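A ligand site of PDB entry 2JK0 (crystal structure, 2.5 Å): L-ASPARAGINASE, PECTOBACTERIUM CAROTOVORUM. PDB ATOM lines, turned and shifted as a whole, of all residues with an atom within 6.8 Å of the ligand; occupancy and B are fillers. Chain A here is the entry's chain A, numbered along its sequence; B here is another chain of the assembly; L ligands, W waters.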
ATOM      1  N   GLY A  11     -21.976  34.432  -5.788  1.00  0.00           N
ATOM      2  CA  GLY A  11     -21.137  33.340  -5.325  1.00  0.00           C
ATOM      3  C   GLY A  11     -20.255  32.844  -6.440  1.00  0.00           C
ATOM      4  O   GLY A  11     -19.578  33.645  -7.074  1.00  0.00           O
ATOM      5  N   GLY A  12     -20.268  31.538  -6.667  1.00  0.00           N
ATOM      6  CA  GLY A  12     -19.571  30.948  -7.805  1.00  0.00           C
ATOM      7  C   GLY A  12     -18.090  30.725  -7.581  1.00  0.00           C
ATOM      8  O   GLY A  12     -17.526  31.164  -6.580  1.00  0.00           O
ATOM      9  N   THR A  13     -17.453  30.012  -8.514  1.00  0.00           N
ATOM     10  CA  THR A  13     -16.014  29.784  -8.473  1.00  0.00           C
ATOM     11  C   THR A  13     -15.174  31.088  -8.542  1.00  0.00           C
ATOM     12  O   THR A  13     -14.101  31.174  -7.931  1.00  0.00           O
ATOM     13  CB  THR A  13     -15.601  28.756  -9.533  1.00  0.00           C
ATOM     14  OG1 THR A  13     -16.251  27.512  -9.222  1.00  0.00           O
ATOM     15  CG2 THR A  13     -14.118  28.518  -9.541  1.00  0.00           C
ATOM     16  N   ILE A  14     -15.650  32.103  -9.265  1.00  0.00           N
ATOM     17  CA  ILE A  14     -14.989  33.405  -9.230  1.00  0.00           C
ATOM     18  C   ILE A  14     -14.624  33.831  -7.793  1.00  0.00           C
ATOM     19  O   ILE A  14     -13.671  34.595  -7.577  1.00  0.00           O
ATOM     20  CB  ILE A  14     -15.837  34.492  -9.901  1.00  0.00           C
ATOM     21  CG1 ILE A  14     -14.964  35.701 -10.257  1.00  0.00           C
ATOM     22  CG2 ILE A  14     -17.089  34.838  -9.040  1.00  0.00           C
ATOM     23  CD1 ILE A  14     -15.643  36.740 -11.127  1.00  0.00           C
ATOM     24  N   ALA A  29     -17.106  26.934  -3.616  1.00  0.00           N
ATOM     25  CA  ALA A  29     -17.693  28.037  -4.366  1.00  0.00           C
ATOM     26  C   ALA A  29     -18.454  28.965  -3.436  1.00  0.00           C
ATOM     27  O   ALA A  29     -19.171  28.517  -2.551  1.00  0.00           O
ATOM     28  N   GLY A  30     -18.287  30.274  -3.662  1.00  0.00           N
ATOM     29  CA  GLY A  30     -18.934  31.316  -2.842  1.00  0.00           C
ATOM     30  C   GLY A  30     -18.381  31.437  -1.422  1.00  0.00           C
ATOM     31  O   GLY A  30     -19.107  31.842  -0.505  1.00  0.00           O
ATOM     32  N   ILE A  58     -23.766  31.381  -3.122  1.00  0.00           N
ATOM     33  CA  ILE A  58     -23.997  29.982  -3.462  1.00  0.00           C
ATOM     34  C   ILE A  58     -23.193  29.598  -4.695  1.00  0.00           C
ATOM     35  O   ILE A  58     -22.721  30.462  -5.424  1.00  0.00           O
ATOM     36  CB  ILE A  58     -25.509  29.694  -3.709  1.00  0.00           C
ATOM     37  CG1 ILE A  58     -26.105  30.671  -4.739  1.00  0.00           C
ATOM     38  CG2 ILE A  58     -26.289  29.753  -2.375  1.00  0.00           C
ATOM     39  CD1 ILE A  58     -27.467  30.287  -5.309  1.00  0.00           C
ATOM     40  N   GLY A  59     -23.005  28.298  -4.903  1.00  0.00           N
ATOM     41  CA  GLY A  59     -22.517  27.796  -6.170  1.00  0.00           C
ATOM     42  C   GLY A  59     -23.702  27.827  -7.122  1.00  0.00           C
ATOM     43  O   GLY A  59     -24.824  27.525  -6.702  1.00  0.00           O
ATOM     44  N   SER A  60     -23.483  28.189  -8.386  1.00  0.00           N
ATOM     45  CA  SER A  60     -24.605  28.384  -9.325  1.00  0.00           C
ATOM     46  C   SER A  60     -25.416  27.133  -9.672  1.00  0.00           C
ATOM     47  O   SER A  60     -26.506  27.258 -10.217  1.00  0.00           O
ATOM     48  CB  SER A  60     -24.192  29.163 -10.578  1.00  0.00           C
ATOM     49  OG  SER A  60     -23.659  28.290 -11.570  1.00  0.00           O
ATOM     50  N   GLU A  61     -24.891  25.950  -9.351  1.00  0.00           N
ATOM     51  CA  GLU A  61     -25.662  24.685  -9.353  1.00  0.00           C
ATOM     52  C   GLU A  61     -26.933  24.858  -8.555  1.00  0.00           C
ATOM     53  O   GLU A  61     -27.970  24.344  -8.916  1.00  0.00           O
ATOM     54  CB  GLU A  61     -24.909  23.549  -8.652  1.00  0.00           C
ATOM     55  CG  GLU A  61     -23.444  23.542  -8.849  1.00  0.00           C
ATOM     56  CD  GLU A  61     -22.710  24.347  -7.807  1.00  0.00           C
ATOM     57  OE1 GLU A  61     -22.205  25.415  -8.165  1.00  0.00           O
ATOM     58  OE2 GLU A  61     -22.639  23.888  -6.633  1.00  0.00           O
ATOM     59  N   ASN A  62     -26.828  25.564  -7.432  1.00  0.00           N
ATOM     60  CA  ASN A  62     -27.971  25.799  -6.571  1.00  0.00           C
ATOM     61  C   ASN A  62     -28.679  27.141  -6.788  1.00  0.00           C
ATOM     62  O   ASN A  62     -29.420  27.598  -5.929  1.00  0.00           O
ATOM     63  CB  ASN A  62     -27.572  25.640  -5.101  1.00  0.00           C
ATOM     64  CG  ASN A  62     -27.129  24.238  -4.774  1.00  0.00           C
ATOM     65  OD1 ASN A  62     -27.928  23.311  -4.728  1.00  0.00           O
ATOM     66  ND2 ASN A  62     -25.830  24.069  -4.524  1.00  0.00           N
ATOM     67  N   HIS A  91     -20.903  35.386 -10.503  1.00  0.00           N
ATOM     68  CA  HIS A  91     -21.814  34.282 -10.645  1.00  0.00           C
ATOM     69  C   HIS A  91     -21.047  33.014 -11.008  1.00  0.00           C
ATOM     70  O   HIS A  91     -19.918  33.077 -11.521  1.00  0.00           O
ATOM     71  CB  HIS A  91     -22.807  34.654 -11.741  1.00  0.00           C
ATOM     72  CG  HIS A  91     -23.988  33.737 -11.855  1.00  0.00           C
ATOM     73  ND1 HIS A  91     -25.264  34.142 -11.569  1.00  0.00           N
ATOM     74  CD2 HIS A  91     -24.081  32.451 -12.276  1.00  0.00           C
ATOM     75  CE1 HIS A  91     -26.099  33.141 -11.777  1.00  0.00           C
ATOM     76  NE2 HIS A  91     -25.406  32.102 -12.207  1.00  0.00           N
ATOM     77  N   GLY A  92     -21.652  31.858 -10.732  1.00  0.00           N
ATOM     78  CA  GLY A  92     -21.112  30.572 -11.156  1.00  0.00           C
ATOM     79  C   GLY A  92     -21.210  30.399 -12.653  1.00  0.00           C
ATOM     80  O   GLY A  92     -21.925  31.147 -13.323  1.00  0.00           O
ATOM     81  N   THR A  93     -20.475  29.431 -13.195  1.00  0.00           N
ATOM     82  CA  THR A  93     -20.554  29.126 -14.604  1.00  0.00           C
ATOM     83  C   THR A  93     -21.596  28.024 -14.834  1.00  0.00           C
ATOM     84  O   THR A  93     -22.268  27.999 -15.851  1.00  0.00           O
ATOM     85  CB  THR A  93     -19.198  28.693 -15.188  1.00  0.00           C
ATOM     86  OG1 THR A  93     -18.745  27.485 -14.563  1.00  0.00           O
ATOM     87  CG2 THR A  93     -18.143  29.775 -15.027  1.00  0.00           C
ATOM     88  N   ASP A  94     -21.763  27.132 -13.868  1.00  0.00           N
ATOM     89  CA  ASP A  94     -22.622  25.954 -14.066  1.00  0.00           C
ATOM     90  C   ASP A  94     -24.020  26.249 -14.604  1.00  0.00           C
ATOM     91  O   ASP A  94     -24.610  25.439 -15.322  1.00  0.00           O
ATOM     92  CB  ASP A  94     -22.712  25.156 -12.784  1.00  0.00           C
ATOM     93  CG  ASP A  94     -21.404  24.479 -12.458  1.00  0.00           C
ATOM     94  OD1 ASP A  94     -20.623  24.325 -13.421  1.00  0.00           O
ATOM     95  OD2 ASP A  94     -21.183  24.123 -11.266  1.00  0.00           O
ATOM     96  N   THR A  95     -24.500  27.443 -14.283  1.00  0.00           N
ATOM     97  CA  THR A  95     -25.851  27.825 -14.534  1.00  0.00           C
ATOM     98  C   THR A  95     -25.874  29.241 -15.167  1.00  0.00           C
ATOM     99  O   THR A  95     -26.929  29.887 -15.272  1.00  0.00           O
ATOM    100  CB  THR A  95     -26.623  27.733 -13.209  1.00  0.00           C
ATOM    101  OG1 THR A  95     -27.799  26.950 -13.393  1.00  0.00           O
ATOM    102  CG2 THR A  95     -26.959  29.090 -12.615  1.00  0.00           C
ATOM    103  N   LEU A  96     -24.710  29.691 -15.627  1.00  0.00           N
ATOM    104  CA  LEU A  96     -24.604  30.989 -16.265  1.00  0.00           C
ATOM    105  C   LEU A  96     -25.295  30.959 -17.634  1.00  0.00           C
ATOM    106  O   LEU A  96     -25.408  31.982 -18.295  1.00  0.00           O
ATOM    107  CB  LEU A  96     -23.136  31.395 -16.450  1.00  0.00           C
ATOM    108  CG  LEU A  96     -22.549  32.708 -15.936  1.00  0.00           C
ATOM    109  CD1 LEU A  96     -21.656  33.247 -17.016  1.00  0.00           C
ATOM    110  CD2 LEU A  96     -23.556  33.768 -15.514  1.00  0.00           C
ATOM    111  N   ALA A 117     -17.815  35.554 -14.443  1.00  0.00           N
ATOM    112  CA  ALA A 117     -17.576  34.287 -13.777  1.00  0.00           C
ATOM    113  C   ALA A 117     -16.134  33.888 -13.978  1.00  0.00           C
ATOM    114  O   ALA A 117     -15.398  34.515 -14.736  1.00  0.00           O
ATOM    115  CB  ALA A 117     -18.494  33.219 -14.345  1.00  0.00           C
ATOM    116  N   ALA A 118     -15.741  32.820 -13.299  1.00  0.00           N
ATOM    117  CA  ALA A 118     -14.422  32.272 -13.482  1.00  0.00           C
ATOM    118  C   ALA A 118     -14.517  30.764 -13.513  1.00  0.00           C
ATOM    119  O   ALA A 118     -15.308  30.171 -12.801  1.00  0.00           O
ATOM    120  CB  ALA A 118     -13.488  32.732 -12.354  1.00  0.00           C
ATOM    121  N   MET A 119     -13.698  30.138 -14.341  1.00  0.00           N
ATOM    122  CA  MET A 119     -13.653  28.675 -14.387  1.00  0.00           C
ATOM    123  C   MET A 119     -12.673  28.112 -13.370  1.00  0.00           C
ATOM    124  O   MET A 119     -12.731  26.935 -13.040  1.00  0.00           O
ATOM    125  CB  MET A 119     -13.296  28.210 -15.795  1.00  0.00           C
ATOM    126  CG  MET A 119     -14.450  28.344 -16.777  1.00  0.00           C
ATOM    127  SD  MET A 119     -15.854  27.256 -16.378  1.00  0.00           S
ATOM    128  CE  MET A 119     -15.194  25.667 -16.852  1.00  0.00           C
ATOM    129  N   ARG A 120     -11.789  28.979 -12.870  1.00  0.00           N
ATOM    130  CA  ARG A 120     -10.780  28.621 -11.886  1.00  0.00           C
ATOM    131  C   ARG A 120     -10.985  29.391 -10.595  1.00  0.00           C
ATOM    132  O   ARG A 120     -11.294  30.590 -10.647  1.00  0.00           O
ATOM    133  CB  ARG A 120      -9.387  28.934 -12.419  1.00  0.00           C
ATOM    134  CG  ARG A 120      -8.806  27.914 -13.320  1.00  0.00           C
ATOM    135  CD  ARG A 120      -7.511  28.430 -13.872  1.00  0.00           C
ATOM    136  NE  ARG A 120      -7.133  27.688 -15.083  1.00  0.00           N
ATOM    137  CZ  ARG A 120      -6.143  28.019 -15.896  1.00  0.00           C
ATOM    138  NH1 ARG A 120      -5.419  29.114 -15.650  1.00  0.00           N
ATOM    139  NH2 ARG A 120      -5.891  27.271 -16.958  1.00  0.00           N
ATOM    140  N   LYS A 166     -22.198  27.713 -21.459  1.00  0.00           N
ATOM    141  CA  LYS A 166     -21.085  26.817 -21.124  1.00  0.00           C
ATOM    142  C   LYS A 166     -21.026  25.641 -22.128  1.00  0.00           C
ATOM    143  O   LYS A 166     -21.893  24.773 -22.111  1.00  0.00           O
ATOM    144  CB  LYS A 166     -21.259  26.327 -19.670  1.00  0.00           C
ATOM    145  CG  LYS A 166     -20.008  25.751 -19.021  1.00  0.00           C
ATOM    146  CD  LYS A 166     -20.123  25.623 -17.502  1.00  0.00           C
ATOM    147  CE  LYS A 166     -18.904  24.865 -16.968  1.00  0.00           C
ATOM    148  NZ  LYS A 166     -18.768  24.844 -15.483  1.00  0.00           N
ATOM    149  N   MET B 248     -25.101  20.092 -14.664  1.00  0.00           N
ATOM    150  CA  MET B 248     -24.804  21.498 -14.871  1.00  0.00           C
ATOM    151  C   MET B 248     -23.272  21.631 -14.905  1.00  0.00           C
ATOM    152  O   MET B 248     -22.590  21.155 -13.986  1.00  0.00           O
ATOM    153  CB  MET B 248     -25.406  22.336 -13.744  1.00  0.00           C
ATOM    154  CG  MET B 248     -26.938  22.353 -13.754  1.00  0.00           C
ATOM    155  SD  MET B 248     -27.725  23.141 -12.327  1.00  0.00           S
ATOM    156  CE  MET B 248     -27.614  21.814 -11.100  1.00  0.00           C
ATOM    157  N   SER B 252     -22.032  19.086 -12.014  1.00  0.00           N
ATOM    158  CA  SER B 252     -22.364  19.671 -10.734  1.00  0.00           C
ATOM    159  C   SER B 252     -23.823  19.395 -10.402  1.00  0.00           C
ATOM    160  O   SER B 252     -24.708  19.553 -11.264  1.00  0.00           O
ATOM    161  CB  SER B 252     -22.114  21.179 -10.712  1.00  0.00           C
ATOM    162  OG  SER B 252     -20.784  21.517 -11.054  1.00  0.00           O
HETATM  163  N1  LIG L   1     -19.649  25.090  -9.498  1.00  0.00           N
HETATM  164  C1  LIG L   1     -19.267  26.483  -9.832  1.00  0.00           C
HETATM  165  C2  LIG L   1     -20.542  27.343  -9.845  1.00  0.00           C
HETATM  166  O1  LIG L   1     -21.340  27.265 -10.788  1.00  0.00           O
HETATM  167  C3  LIG L   1     -18.563  26.533 -11.191  1.00  0.00           C
HETATM  168  C4  LIG L   1     -18.034  27.921 -11.544  1.00  0.00           C
HETATM  169  O2  LIG L   1     -17.054  28.009 -12.293  1.00  0.00           O
HETATM  170  O3  LIG L   1     -18.587  28.942 -11.083  1.00  0.00           O
HETATM  171  O4  LIG L   1     -20.783  28.128  -8.931  1.00  0.00           O
HETATM  172  O   HOH W   1     -15.559  25.836 -12.953  1.00  0.00           O
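O1 of the ligand is in hydrogen-bond range of N of Asp 94, 3.1 Å away.
The side-chain carboxylate (OD2) of Asp 94 is in salt-bridge range of a nitrogen (N1) of the ligand, 2.5 Å away.
The backbone NH (N) of Ser 60 lies within hydrogen-bond range of an oxygen (O4) of the ligand, 2.8 Å away.
OG of Ser 60 lies within hydrogen-bond range of O1 of the ligand (2.7 Å).
An oxygen (O2) of the ligand sits close to the backbone carbonyl oxygen (O) of Ala 118, at 2.8 Å.
N of Thr 93 lies within hydrogen-bond range of O3 of the ligand, at 2.9 Å.
The side-chain hydroxyl of Thr 93 lies within hydrogen-bond range of an oxygen (O2) of the ligand, at 2.9 Å.
The side-chain carboxylate of Glu 61 lies within salt-bridge range of a nitrogen (N1) of the ligand (2.9 Å).
An oxygen (O3) of the ligand lies within hydrogen-bond range of the backbone NH (N) of Thr 13, 3.0 Å away.
O2 of the ligand lies close to OG1 of Thr 13 (3.2 Å).
The backbone NH (N) of Asp 94 lies within hydrogen-bond range of the side-chain hydroxyl (OG) of Ser 60 (3.2 Å).
OG of Ser 252 of chain B lies within hydrogen-bond range of OD2 of Asp 94, at 2.6 Å.
The side-chain carboxylate (OD1) of Asp 94 lies within salt-bridge range of the side-chain amino group (NZ) of Lys 166 (2.8 Å).
The backbone NH (N) of Thr 95 lies within hydrogen-bond range of the side-chain hydroxyl (OG) of Ser 60, at 3.0 Å.
OG1 of Thr 93 lies within hydrogen-bond range of SD of Met 119.
OG1 of Thr 93 sits at hydrogen-bond distance from NZ of Lys 166, at 2.8 Å.
N of Gly 12 is in hydrogen-bond range of O of Ile 58.
The backbone carbonyl oxygen (O) of Gly 12 sits at hydrogen-bond distance from the backbone NH (N) of Gly 30 (3.1 Å).
Gly 12 touches the ligand.
Gly 59 touches the ligand (CA to O4, 3.3 Å).
Gly 92 touches the ligand.
Nine residues have an atom within 4 Å of the ligand: Gly 12, Thr 13, Gly 59, Ser 60, Glu 61, Gly 92, Thr 93, Asp 94 and Ala 118.
Along chain A the residues within 4 Å of the ligand span positions 12 to 118.
The nearest printed residue that does not touch the ligand is Met 119 (4.05 Å).
Water W1 bridges O2 of the ligand (2.7 Å) and O of Met 119 (3.0 Å).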
